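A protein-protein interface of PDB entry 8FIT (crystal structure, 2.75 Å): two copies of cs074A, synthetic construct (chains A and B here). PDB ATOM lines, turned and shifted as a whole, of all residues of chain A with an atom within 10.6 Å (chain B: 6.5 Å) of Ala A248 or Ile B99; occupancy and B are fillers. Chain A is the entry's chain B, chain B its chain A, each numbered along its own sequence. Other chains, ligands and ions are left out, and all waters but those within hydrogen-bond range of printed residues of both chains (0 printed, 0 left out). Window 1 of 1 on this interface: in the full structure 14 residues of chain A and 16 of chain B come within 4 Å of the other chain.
Printed residues of chain B within 4 Å of Ala A248: Leu B73, Lys B80 and Ile B99.
Ile B99 touches just these residues of chain A: Ala A248 and Val A249.
No residue of chain A comes within 4 Å of Ala B76.
No residue of chain A comes within 4 Å of Ala B95.
No residue of chain A comes within 4 Å of Ala B96.
No residue of chain A comes within 4 Å of Ala B100.
Ala B102 touches one residue of chain A.
Of chain A, only Leu A245 comes within 4 Å of Ile B103.
Of the printed residues of chain A, Leu B73 touches Leu A244 (3.6 Å), Leu A245 (3.6 Å) and Ala A248 (3.9 Å).
Printed residues of chain B within 4 Å of Leu A244: Leu B73 (3.6 Å).
Printed residues of chain B within 4 Å of Val A255: Lys B80 (3.9 Å).
Printed residues of chain A within 4 Å of Ala B125: Val A249.
The nearest printed residue of chain A that does not touch Ala B125 is Glu A246 (4.4 Å).
Of the 17 printed residues of chain A, 6 touch a printed residue of chain B.
Hydrophobic or aromatic side chains of chain B that line the printed part of chain A: Leu B73, Ile B99, Ala B102 and Ile B103.
Among the printed residues, no Asp or Glu carboxylate lies within 4 Å of a Lys or Arg side-chain nitrogen of the other chain.
No position is printed for both chains.
Of the 11 pairs that touch across the chains among the printed residues, none has its exchanged pair printed and touching as well.
Leu B73 touches Leu A245 (CD1 to CD1, 3.6 Å).
Ala B102 touches Leu A245 (O to CD2, 3.3 Å).
Leu A245 touches Ile B103.
Leu B73 touches Ala A248 (CD2 to CB, 3.9 Å).
CE of Lys B80 touches O of Ala A248, at 3.7 Å.
O of Ala A248 touches CD1 of Ile B99, 3.5 Å away.
Ile B99 touches Val A249.
CG1 of Val A249 touches O of Ala B125, 3.98 Å away.
CD2 of Leu A252 touches NZ of Lys B80 (3.3 Å).
CG1 of Val A255 touches O of Lys B80, 3.9 Å away.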
ATOM      1  N   GLU A 240      -2.338  -7.626   8.158  1.00  0.00           N
ATOM      2  CA  GLU A 240      -1.629  -7.083   7.005  1.00  0.00           C
ATOM      3  C   GLU A 240      -0.185  -6.717   7.317  1.00  0.00           C
ATOM      4  O   GLU A 240       0.552  -6.348   6.397  1.00  0.00           O
ATOM      5  CB  GLU A 240      -2.363  -5.855   6.463  1.00  0.00           C
ATOM      6  CG  GLU A 240      -2.245  -4.620   7.341  1.00  0.00           C
ATOM      7  CD  GLU A 240      -2.942  -3.413   6.744  1.00  0.00           C
ATOM      8  OE1 GLU A 240      -3.891  -3.603   5.955  1.00  0.00           O
ATOM      9  OE2 GLU A 240      -2.535  -2.275   7.058  1.00  0.00           O
ATOM     10  N   ALA A 241       0.235  -6.804   8.582  1.00  0.00           N
ATOM     11  CA  ALA A 241       1.626  -6.542   8.927  1.00  0.00           C
ATOM     12  C   ALA A 241       2.577  -7.537   8.277  1.00  0.00           C
ATOM     13  O   ALA A 241       3.762  -7.227   8.115  1.00  0.00           O
ATOM     14  CB  ALA A 241       1.806  -6.564  10.446  1.00  0.00           C
ATOM     15  N   ALA A 242       2.087  -8.722   7.902  1.00  0.00           N
ATOM     16  CA  ALA A 242       2.932  -9.688   7.207  1.00  0.00           C
ATOM     17  C   ALA A 242       3.501  -9.098   5.924  1.00  0.00           C
ATOM     18  O   ALA A 242       4.685  -9.281   5.618  1.00  0.00           O
ATOM     19  CB  ALA A 242       2.139 -10.962   6.910  1.00  0.00           C
ATOM     20  N   ARG A 243       2.673  -8.382   5.160  1.00  0.00           N
ATOM     21  CA  ARG A 243       3.159  -7.665   3.989  1.00  0.00           C
ATOM     22  C   ARG A 243       3.891  -6.381   4.356  1.00  0.00           C
ATOM     23  O   ARG A 243       4.698  -5.891   3.558  1.00  0.00           O
ATOM     24  CB  ARG A 243       1.999  -7.340   3.046  1.00  0.00           C
ATOM     25  CG  ARG A 243       2.014  -8.123   1.743  1.00  0.00           C
ATOM     26  CD  ARG A 243       1.805  -9.609   1.981  1.00  0.00           C
ATOM     27  NE  ARG A 243       1.791 -10.358   0.729  1.00  0.00           N
ATOM     28  CZ  ARG A 243       1.544 -11.658   0.638  1.00  0.00           C
ATOM     29  NH1 ARG A 243       1.280 -12.389   1.709  1.00  0.00           N
ATOM     30  NH2 ARG A 243       1.559 -12.239  -0.559  1.00  0.00           N
ATOM     31  N   LEU A 244       3.625  -5.826   5.539  1.00  0.00           N
ATOM     32  CA  LEU A 244       4.313  -4.616   5.970  1.00  0.00           C
ATOM     33  C   LEU A 244       5.720  -4.922   6.470  1.00  0.00           C
ATOM     34  O   LEU A 244       6.646  -4.133   6.249  1.00  0.00           O
ATOM     35  CB  LEU A 244       3.489  -3.912   7.050  1.00  0.00           C
ATOM     36  CG  LEU A 244       4.143  -2.836   7.921  1.00  0.00           C
ATOM     37  CD1 LEU A 244       4.718  -1.702   7.089  1.00  0.00           C
ATOM     38  CD2 LEU A 244       3.145  -2.300   8.939  1.00  0.00           C
ATOM     39  N   LEU A 245       5.904  -6.065   7.134  1.00  0.00           N
ATOM     40  CA  LEU A 245       7.223  -6.407   7.655  1.00  0.00           C
ATOM     41  C   LEU A 245       8.180  -6.807   6.538  1.00  0.00           C
ATOM     42  O   LEU A 245       9.371  -6.478   6.590  1.00  0.00           O
ATOM     43  CB  LEU A 245       7.109  -7.525   8.692  1.00  0.00           C
ATOM     44  CG  LEU A 245       7.008  -7.089  10.156  1.00  0.00           C
ATOM     45  CD1 LEU A 245       5.670  -6.436  10.465  1.00  0.00           C
ATOM     46  CD2 LEU A 245       7.245  -8.270  11.073  1.00  0.00           C
ATOM     47  N   GLU A 246       7.684  -7.519   5.522  1.00  0.00           N
ATOM     48  CA  GLU A 246       8.545  -7.906   4.410  1.00  0.00           C
ATOM     49  C   GLU A 246       9.028  -6.701   3.615  1.00  0.00           C
ATOM     50  O   GLU A 246      10.068  -6.786   2.952  1.00  0.00           O
ATOM     51  CB  GLU A 246       7.819  -8.898   3.495  1.00  0.00           C
ATOM     52  CG  GLU A 246       6.588  -8.349   2.791  1.00  0.00           C
ATOM     53  CD  GLU A 246       6.906  -7.736   1.439  1.00  0.00           C
ATOM     54  OE1 GLU A 246       8.046  -7.906   0.959  1.00  0.00           O
ATOM     55  OE2 GLU A 246       6.013  -7.084   0.857  1.00  0.00           O
ATOM     56  N   LEU A 247       8.298  -5.585   3.661  1.00  0.00           N
ATOM     57  CA  LEU A 247       8.806  -4.344   3.091  1.00  0.00           C
ATOM     58  C   LEU A 247       9.873  -3.719   3.979  1.00  0.00           C
ATOM     59  O   LEU A 247      10.801  -3.085   3.469  1.00  0.00           O
ATOM     60  CB  LEU A 247       7.662  -3.352   2.870  1.00  0.00           C
ATOM     61  CG  LEU A 247       6.627  -3.703   1.800  1.00  0.00           C
ATOM     62  CD1 LEU A 247       5.567  -2.615   1.707  1.00  0.00           C
ATOM     63  CD2 LEU A 247       7.302  -3.915   0.456  1.00  0.00           C
ATOM     64  N   ALA A 248       9.758  -3.891   5.298  1.00  0.00           N
ATOM     65  CA  ALA A 248      10.764  -3.348   6.205  1.00  0.00           C
ATOM     66  C   ALA A 248      12.089  -4.085   6.066  1.00  0.00           C
ATOM     67  O   ALA A 248      13.157  -3.464   6.100  1.00  0.00           O
ATOM     68  CB  ALA A 248      10.259  -3.409   7.646  1.00  0.00           C
ATOM     69  N   VAL A 249      12.042  -5.410   5.909  1.00  0.00           N
ATOM     70  CA  VAL A 249      13.274  -6.162   5.694  1.00  0.00           C
ATOM     71  C   VAL A 249      13.836  -5.871   4.310  1.00  0.00           C
ATOM     72  O   VAL A 249      15.050  -5.964   4.093  1.00  0.00           O
ATOM     73  CB  VAL A 249      13.040  -7.671   5.908  1.00  0.00           C
ATOM     74  CG1 VAL A 249      12.298  -7.916   7.207  1.00  0.00           C
ATOM     75  CG2 VAL A 249      12.283  -8.279   4.737  1.00  0.00           C
ATOM     76  N   GLU A 250      12.975  -5.508   3.357  1.00  0.00           N
ATOM     77  CA  GLU A 250      13.446  -5.134   2.030  1.00  0.00           C
ATOM     78  C   GLU A 250      13.880  -3.676   1.984  1.00  0.00           C
ATOM     79  O   GLU A 250      14.766  -3.321   1.199  1.00  0.00           O
ATOM     80  CB  GLU A 250      12.354  -5.404   0.992  1.00  0.00           C
ATOM     81  CG  GLU A 250      12.857  -6.036  -0.298  1.00  0.00           C
ATOM     82  CD  GLU A 250      13.585  -5.052  -1.191  1.00  0.00           C
ATOM     83  OE1 GLU A 250      13.258  -3.847  -1.140  1.00  0.00           O
ATOM     84  OE2 GLU A 250      14.482  -5.483  -1.946  1.00  0.00           O
ATOM     85  N   ASP A 251      13.273  -2.823   2.814  1.00  0.00           N
ATOM     86  CA  ASP A 251      13.750  -1.450   2.939  1.00  0.00           C
ATOM     87  C   ASP A 251      15.147  -1.416   3.543  1.00  0.00           C
ATOM     88  O   ASP A 251      16.011  -0.662   3.080  1.00  0.00           O
ATOM     89  CB  ASP A 251      12.777  -0.631   3.788  1.00  0.00           C
ATOM     90  CG  ASP A 251      13.132   0.843   3.829  1.00  0.00           C
ATOM     91  OD1 ASP A 251      13.925   1.293   2.975  1.00  0.00           O
ATOM     92  OD2 ASP A 251      12.618   1.553   4.719  1.00  0.00           O
ATOM     93  N   LEU A 252      15.388  -2.229   4.574  1.00  0.00           N
ATOM     94  CA  LEU A 252      16.718  -2.296   5.169  1.00  0.00           C
ATOM     95  C   LEU A 252      17.739  -2.857   4.187  1.00  0.00           C
ATOM     96  O   LEU A 252      18.931  -2.547   4.291  1.00  0.00           O
ATOM     97  CB  LEU A 252      16.678  -3.138   6.445  1.00  0.00           C
ATOM     98  CG  LEU A 252      17.936  -3.142   7.316  1.00  0.00           C
ATOM     99  CD1 LEU A 252      18.332  -1.723   7.685  1.00  0.00           C
ATOM    100  CD2 LEU A 252      17.723  -3.983   8.565  1.00  0.00           C
ATOM    101  N   LYS A 253      17.294  -3.677   3.231  1.00  0.00           N
ATOM    102  CA  LYS A 253      18.195  -4.169   2.194  1.00  0.00           C
ATOM    103  C   LYS A 253      18.746  -3.020   1.359  1.00  0.00           C
ATOM    104  O   LYS A 253      19.959  -2.923   1.137  1.00  0.00           O
ATOM    105  CB  LYS A 253      17.468  -5.179   1.303  1.00  0.00           C
ATOM    106  CG  LYS A 253      17.354  -6.569   1.899  1.00  0.00           C
ATOM    107  CD  LYS A 253      16.292  -7.400   1.195  1.00  0.00           C
ATOM    108  CE  LYS A 253      16.586  -7.552  -0.287  1.00  0.00           C
ATOM    109  NZ  LYS A 253      15.551  -8.383  -0.960  1.00  0.00           N
ATOM    110  N   LEU A 254      17.864  -2.135   0.890  1.00  0.00           N
ATOM    111  CA  LEU A 254      18.310  -1.018   0.065  1.00  0.00           C
ATOM    112  C   LEU A 254      19.080   0.013   0.880  1.00  0.00           C
ATOM    113  O   LEU A 254      20.003   0.645   0.357  1.00  0.00           O
ATOM    114  CB  LEU A 254      17.112  -0.368  -0.628  1.00  0.00           C
ATOM    115  CG  LEU A 254      16.332  -1.281  -1.577  1.00  0.00           C
ATOM    116  CD1 LEU A 254      15.162  -0.538  -2.204  1.00  0.00           C
ATOM    117  CD2 LEU A 254      17.249  -1.849  -2.650  1.00  0.00           C
ATOM    118  N   VAL A 255      18.721   0.197   2.152  1.00  0.00           N
ATOM    119  CA  VAL A 255      19.460   1.128   3.001  1.00  0.00           C
ATOM    120  C   VAL A 255      20.854   0.590   3.297  1.00  0.00           C
ATOM    121  O   VAL A 255      21.841   1.336   3.274  1.00  0.00           O
ATOM    122  CB  VAL A 255      18.673   1.415   4.293  1.00  0.00           C
ATOM    123  CG1 VAL A 255      19.507   2.252   5.251  1.00  0.00           C
ATOM    124  CG2 VAL A 255      17.365   2.121   3.971  1.00  0.00           C
ATOM    125  N   LEU A 256      20.960  -0.712   3.575  1.00  0.00           N
ATOM    126  CA  LEU A 256      22.271  -1.320   3.779  1.00  0.00           C
ATOM    127  C   LEU A 256      23.114  -1.236   2.513  1.00  0.00           C
ATOM    128  O   LEU A 256      24.308  -0.919   2.571  1.00  0.00           O
ATOM    129  CB  LEU A 256      22.107  -2.774   4.232  1.00  0.00           C
ATOM    130  CG  LEU A 256      23.329  -3.615   4.627  1.00  0.00           C
ATOM    131  CD1 LEU A 256      23.968  -4.297   3.421  1.00  0.00           C
ATOM    132  CD2 LEU A 256      24.355  -2.776   5.376  1.00  0.00           C
ATOM    133  N   LEU B  38      13.286   0.502  22.111  1.00  0.00           N
ATOM    134  CA  LEU B  38      13.498  -0.877  21.682  1.00  0.00           C
ATOM    135  C   LEU B  38      13.497  -1.828  22.872  1.00  0.00           C
ATOM    136  O   LEU B  38      12.848  -2.879  22.838  1.00  0.00           O
ATOM    137  CB  LEU B  38      14.810  -0.988  20.904  1.00  0.00           C
ATOM    138  CG  LEU B  38      15.211  -2.398  20.469  1.00  0.00           C
ATOM    139  CD1 LEU B  38      14.212  -2.960  19.471  1.00  0.00           C
ATOM    140  CD2 LEU B  38      16.615  -2.402  19.890  1.00  0.00           C
ATOM    141  N   LEU B  72       7.252  -1.736  16.894  1.00  0.00           N
ATOM    142  CA  LEU B  72       8.616  -2.195  16.663  1.00  0.00           C
ATOM    143  C   LEU B  72       9.139  -1.732  15.311  1.00  0.00           C
ATOM    144  O   LEU B  72      10.336  -1.455  15.173  1.00  0.00           O
ATOM    145  CB  LEU B  72       8.687  -3.717  16.772  1.00  0.00           C
ATOM    146  CG  LEU B  72       8.793  -4.268  18.195  1.00  0.00           C
ATOM    147  CD1 LEU B  72       8.407  -5.736  18.236  1.00  0.00           C
ATOM    148  CD2 LEU B  72      10.203  -4.072  18.723  1.00  0.00           C
ATOM    149  N   LEU B  73       8.265  -1.639  14.307  1.00  0.00           N
ATOM    150  CA  LEU B  73       8.685  -1.110  13.016  1.00  0.00           C
ATOM    151  C   LEU B  73       8.893   0.396  13.053  1.00  0.00           C
ATOM    152  O   LEU B  73       9.659   0.920  12.238  1.00  0.00           O
ATOM    153  CB  LEU B  73       7.669  -1.469  11.934  1.00  0.00           C
ATOM    154  CG  LEU B  73       7.649  -2.936  11.507  1.00  0.00           C
ATOM    155  CD1 LEU B  73       6.895  -3.083  10.203  1.00  0.00           C
ATOM    156  CD2 LEU B  73       9.062  -3.482  11.375  1.00  0.00           C
ATOM    157  N   ALA B  76      12.328   0.622  14.106  1.00  0.00           N
ATOM    158  CA  ALA B  76      13.129   0.219  12.957  1.00  0.00           C
ATOM    159  C   ALA B  76      13.077   1.267  11.853  1.00  0.00           C
ATOM    160  O   ALA B  76      14.077   1.499  11.167  1.00  0.00           O
ATOM    161  CB  ALA B  76      12.655  -1.137  12.435  1.00  0.00           C
ATOM    162  N   LYS B  80      16.560   3.116  10.674  1.00  0.00           N
ATOM    163  CA  LYS B  80      17.084   3.058   9.312  1.00  0.00           C
ATOM    164  C   LYS B  80      17.332   4.455   8.757  1.00  0.00           C
ATOM    165  O   LYS B  80      18.333   4.686   8.070  1.00  0.00           O
ATOM    166  CB  LYS B  80      16.120   2.292   8.405  1.00  0.00           C
ATOM    167  CG  LYS B  80      15.918   0.844   8.798  1.00  0.00           C
ATOM    168  CD  LYS B  80      14.849   0.186   7.946  1.00  0.00           C
ATOM    169  CE  LYS B  80      14.250  -1.008   8.664  1.00  0.00           C
ATOM    170  NZ  LYS B  80      15.310  -1.844   9.289  1.00  0.00           N
ATOM    171  N   LEU B  94      20.763  -2.186  15.406  1.00  0.00           N
ATOM    172  CA  LEU B  94      19.586  -1.945  16.234  1.00  0.00           C
ATOM    173  C   LEU B  94      18.309  -1.990  15.405  1.00  0.00           C
ATOM    174  O   LEU B  94      17.274  -2.482  15.868  1.00  0.00           O
ATOM    175  CB  LEU B  94      19.711  -0.602  16.956  1.00  0.00           C
ATOM    176  CG  LEU B  94      20.535  -0.541  18.247  1.00  0.00           C
ATOM    177  CD1 LEU B  94      20.108  -1.633  19.215  1.00  0.00           C
ATOM    178  CD2 LEU B  94      22.027  -0.617  17.972  1.00  0.00           C
ATOM    179  N   ALA B  95      18.363  -1.479  14.171  1.00  0.00           N
ATOM    180  CA  ALA B  95      17.200  -1.551  13.292  1.00  0.00           C
ATOM    181  C   ALA B  95      16.859  -2.996  12.954  1.00  0.00           C
ATOM    182  O   ALA B  95      15.680  -3.358  12.854  1.00  0.00           O
ATOM    183  CB  ALA B  95      17.452  -0.747  12.019  1.00  0.00           C
ATOM    184  N   ALA B  96      17.879  -3.839  12.775  1.00  0.00           N
ATOM    185  CA  ALA B  96      17.631  -5.249  12.500  1.00  0.00           C
ATOM    186  C   ALA B  96      17.051  -5.961  13.714  1.00  0.00           C
ATOM    187  O   ALA B  96      16.287  -6.919  13.561  1.00  0.00           O
ATOM    188  CB  ALA B  96      18.920  -5.932  12.045  1.00  0.00           C
ATOM    189  N   GLU B  97      17.399  -5.511  14.923  1.00  0.00           N
ATOM    190  CA  GLU B  97      16.812  -6.096  16.123  1.00  0.00           C
ATOM    191  C   GLU B  97      15.339  -5.729  16.250  1.00  0.00           C
ATOM    192  O   GLU B  97      14.517  -6.566  16.637  1.00  0.00           O
ATOM    193  CB  GLU B  97      17.580  -5.642  17.365  1.00  0.00           C
ATOM    194  CG  GLU B  97      19.044  -6.038  17.379  1.00  0.00           C
ATOM    195  CD  GLU B  97      19.733  -5.657  18.674  1.00  0.00           C
ATOM    196  OE1 GLU B  97      19.027  -5.441  19.682  1.00  0.00           O
ATOM    197  OE2 GLU B  97      20.980  -5.571  18.685  1.00  0.00           O
ATOM    198  N   ALA B  98      14.991  -4.478  15.935  1.00  0.00           N
ATOM    199  CA  ALA B  98      13.595  -4.059  15.999  1.00  0.00           C
ATOM    200  C   ALA B  98      12.730  -4.845  15.024  1.00  0.00           C
ATOM    201  O   ALA B  98      11.565  -5.131  15.318  1.00  0.00           O
ATOM    202  CB  ALA B  98      13.482  -2.560  15.723  1.00  0.00           C
ATOM    203  N   ILE B  99      13.281  -5.202  13.862  1.00  0.00           N
ATOM    204  CA  ILE B  99      12.540  -6.033  12.920  1.00  0.00           C
ATOM    205  C   ILE B  99      12.447  -7.464  13.431  1.00  0.00           C
ATOM    206  O   ILE B  99      11.402  -8.114  13.310  1.00  0.00           O
ATOM    207  CB  ILE B  99      13.193  -5.972  11.527  1.00  0.00           C
ATOM    208  CG1 ILE B  99      12.991  -4.593  10.898  1.00  0.00           C
ATOM    209  CG2 ILE B  99      12.634  -7.056  10.628  1.00  0.00           C
ATOM    210  CD1 ILE B  99      13.454  -4.516   9.462  1.00  0.00           C
ATOM    211  N   ALA B 100      13.534  -7.975  14.015  1.00  0.00           N
ATOM    212  CA  ALA B 100      13.549  -9.353  14.500  1.00  0.00           C
ATOM    213  C   ALA B 100      12.446  -9.589  15.522  1.00  0.00           C
ATOM    214  O   ALA B 100      11.683 -10.556  15.417  1.00  0.00           O
ATOM    215  CB  ALA B 100      14.918  -9.683  15.094  1.00  0.00           C
ATOM    216  N   TRP B 101      12.341  -8.708  16.519  1.00  0.00           N
ATOM    217  CA  TRP B 101      11.265  -8.836  17.495  1.00  0.00           C
ATOM    218  C   TRP B 101       9.907  -8.546  16.870  1.00  0.00           C
ATOM    219  O   TRP B 101       8.885  -9.039  17.361  1.00  0.00           O
ATOM    220  CB  TRP B 101      11.528  -7.917  18.685  1.00  0.00           C
ATOM    221  CG  TRP B 101      12.626  -8.421  19.562  1.00  0.00           C
ATOM    222  CD1 TRP B 101      13.964  -8.207  19.405  1.00  0.00           C
ATOM    223  CD2 TRP B 101      12.484  -9.246  20.725  1.00  0.00           C
ATOM    224  NE1 TRP B 101      14.664  -8.843  20.402  1.00  0.00           N
ATOM    225  CE2 TRP B 101      13.778  -9.486  21.226  1.00  0.00           C
ATOM    226  CE3 TRP B 101      11.387  -9.800  21.393  1.00  0.00           C
ATOM    227  CZ2 TRP B 101      14.006 -10.256  22.366  1.00  0.00           C
ATOM    228  CZ3 TRP B 101      11.616 -10.563  22.523  1.00  0.00           C
ATOM    229  CH2 TRP B 101      12.914 -10.784  22.997  1.00  0.00           C
ATOM    230  N   ALA B 102       9.871  -7.756  15.795  1.00  0.00           N
ATOM    231  CA  ALA B 102       8.628  -7.592  15.053  1.00  0.00           C
ATOM    232  C   ALA B 102       8.251  -8.871  14.319  1.00  0.00           C
ATOM    233  O   ALA B 102       7.062  -9.189  14.199  1.00  0.00           O
ATOM    234  CB  ALA B 102       8.742  -6.425  14.073  1.00  0.00           C
ATOM    235  N   ILE B 103       9.245  -9.614  13.821  1.00  0.00           N
ATOM    236  CA  ILE B 103       8.973 -10.915  13.216  1.00  0.00           C
ATOM    237  C   ILE B 103       8.403 -11.872  14.254  1.00  0.00           C
ATOM    238  O   ILE B 103       7.443 -12.604  13.986  1.00  0.00           O
ATOM    239  CB  ILE B 103      10.248 -11.485  12.566  1.00  0.00           C
ATOM    240  CG1 ILE B 103      10.732 -10.580  11.432  1.00  0.00           C
ATOM    241  CG2 ILE B 103       9.999 -12.896  12.053  1.00  0.00           C
ATOM    242  CD1 ILE B 103       9.851 -10.609  10.207  1.00  0.00           C
ATOM    243  N   GLU B 104       8.983 -11.881  15.457  1.00  0.00           N
ATOM    244  CA  GLU B 104       8.468 -12.742  16.516  1.00  0.00           C
ATOM    245  C   GLU B 104       7.053 -12.341  16.911  1.00  0.00           C
ATOM    246  O   GLU B 104       6.179 -13.199  17.079  1.00  0.00           O
ATOM    247  CB  GLU B 104       9.395 -12.695  17.732  1.00  0.00           C
ATOM    248  CG  GLU B 104      10.812 -13.169  17.462  1.00  0.00           C
ATOM    249  CD  GLU B 104      11.612 -13.357  18.738  1.00  0.00           C
ATOM    250  OE1 GLU B 104      10.992 -13.467  19.817  1.00  0.00           O
ATOM    251  OE2 GLU B 104      12.858 -13.390  18.663  1.00  0.00           O
ATOM    252  N   ALA B 125      10.084 -13.722   5.816  1.00  0.00           N
ATOM    253  CA  ALA B 125      10.727 -12.445   6.104  1.00  0.00           C
ATOM    254  C   ALA B 125      11.890 -12.609   7.074  1.00  0.00           C
ATOM    255  O   ALA B 125      12.863 -11.850   7.006  1.00  0.00           O
ATOM    256  CB  ALA B 125       9.706 -11.454   6.660  1.00  0.00           C
ATOM    257  N   LEU B 129      15.515 -11.245   6.556  1.00  0.00           N
ATOM    258  CA  LEU B 129      16.219 -10.505   7.597  1.00  0.00           C
ATOM    259  C   LEU B 129      17.554 -11.153   7.936  1.00  0.00           C
ATOM    260  O   LEU B 129      18.506 -10.455   8.306  1.00  0.00           O
ATOM    261  CB  LEU B 129      15.347 -10.401   8.847  1.00  0.00           C
ATOM    262  CG  LEU B 129      15.966  -9.703  10.059  1.00  0.00           C
ATOM    263  CD1 LEU B 129      16.165  -8.221   9.787  1.00  0.00           C
ATOM    264  CD2 LEU B 129      15.110  -9.921  11.293  1.00  0.00           C
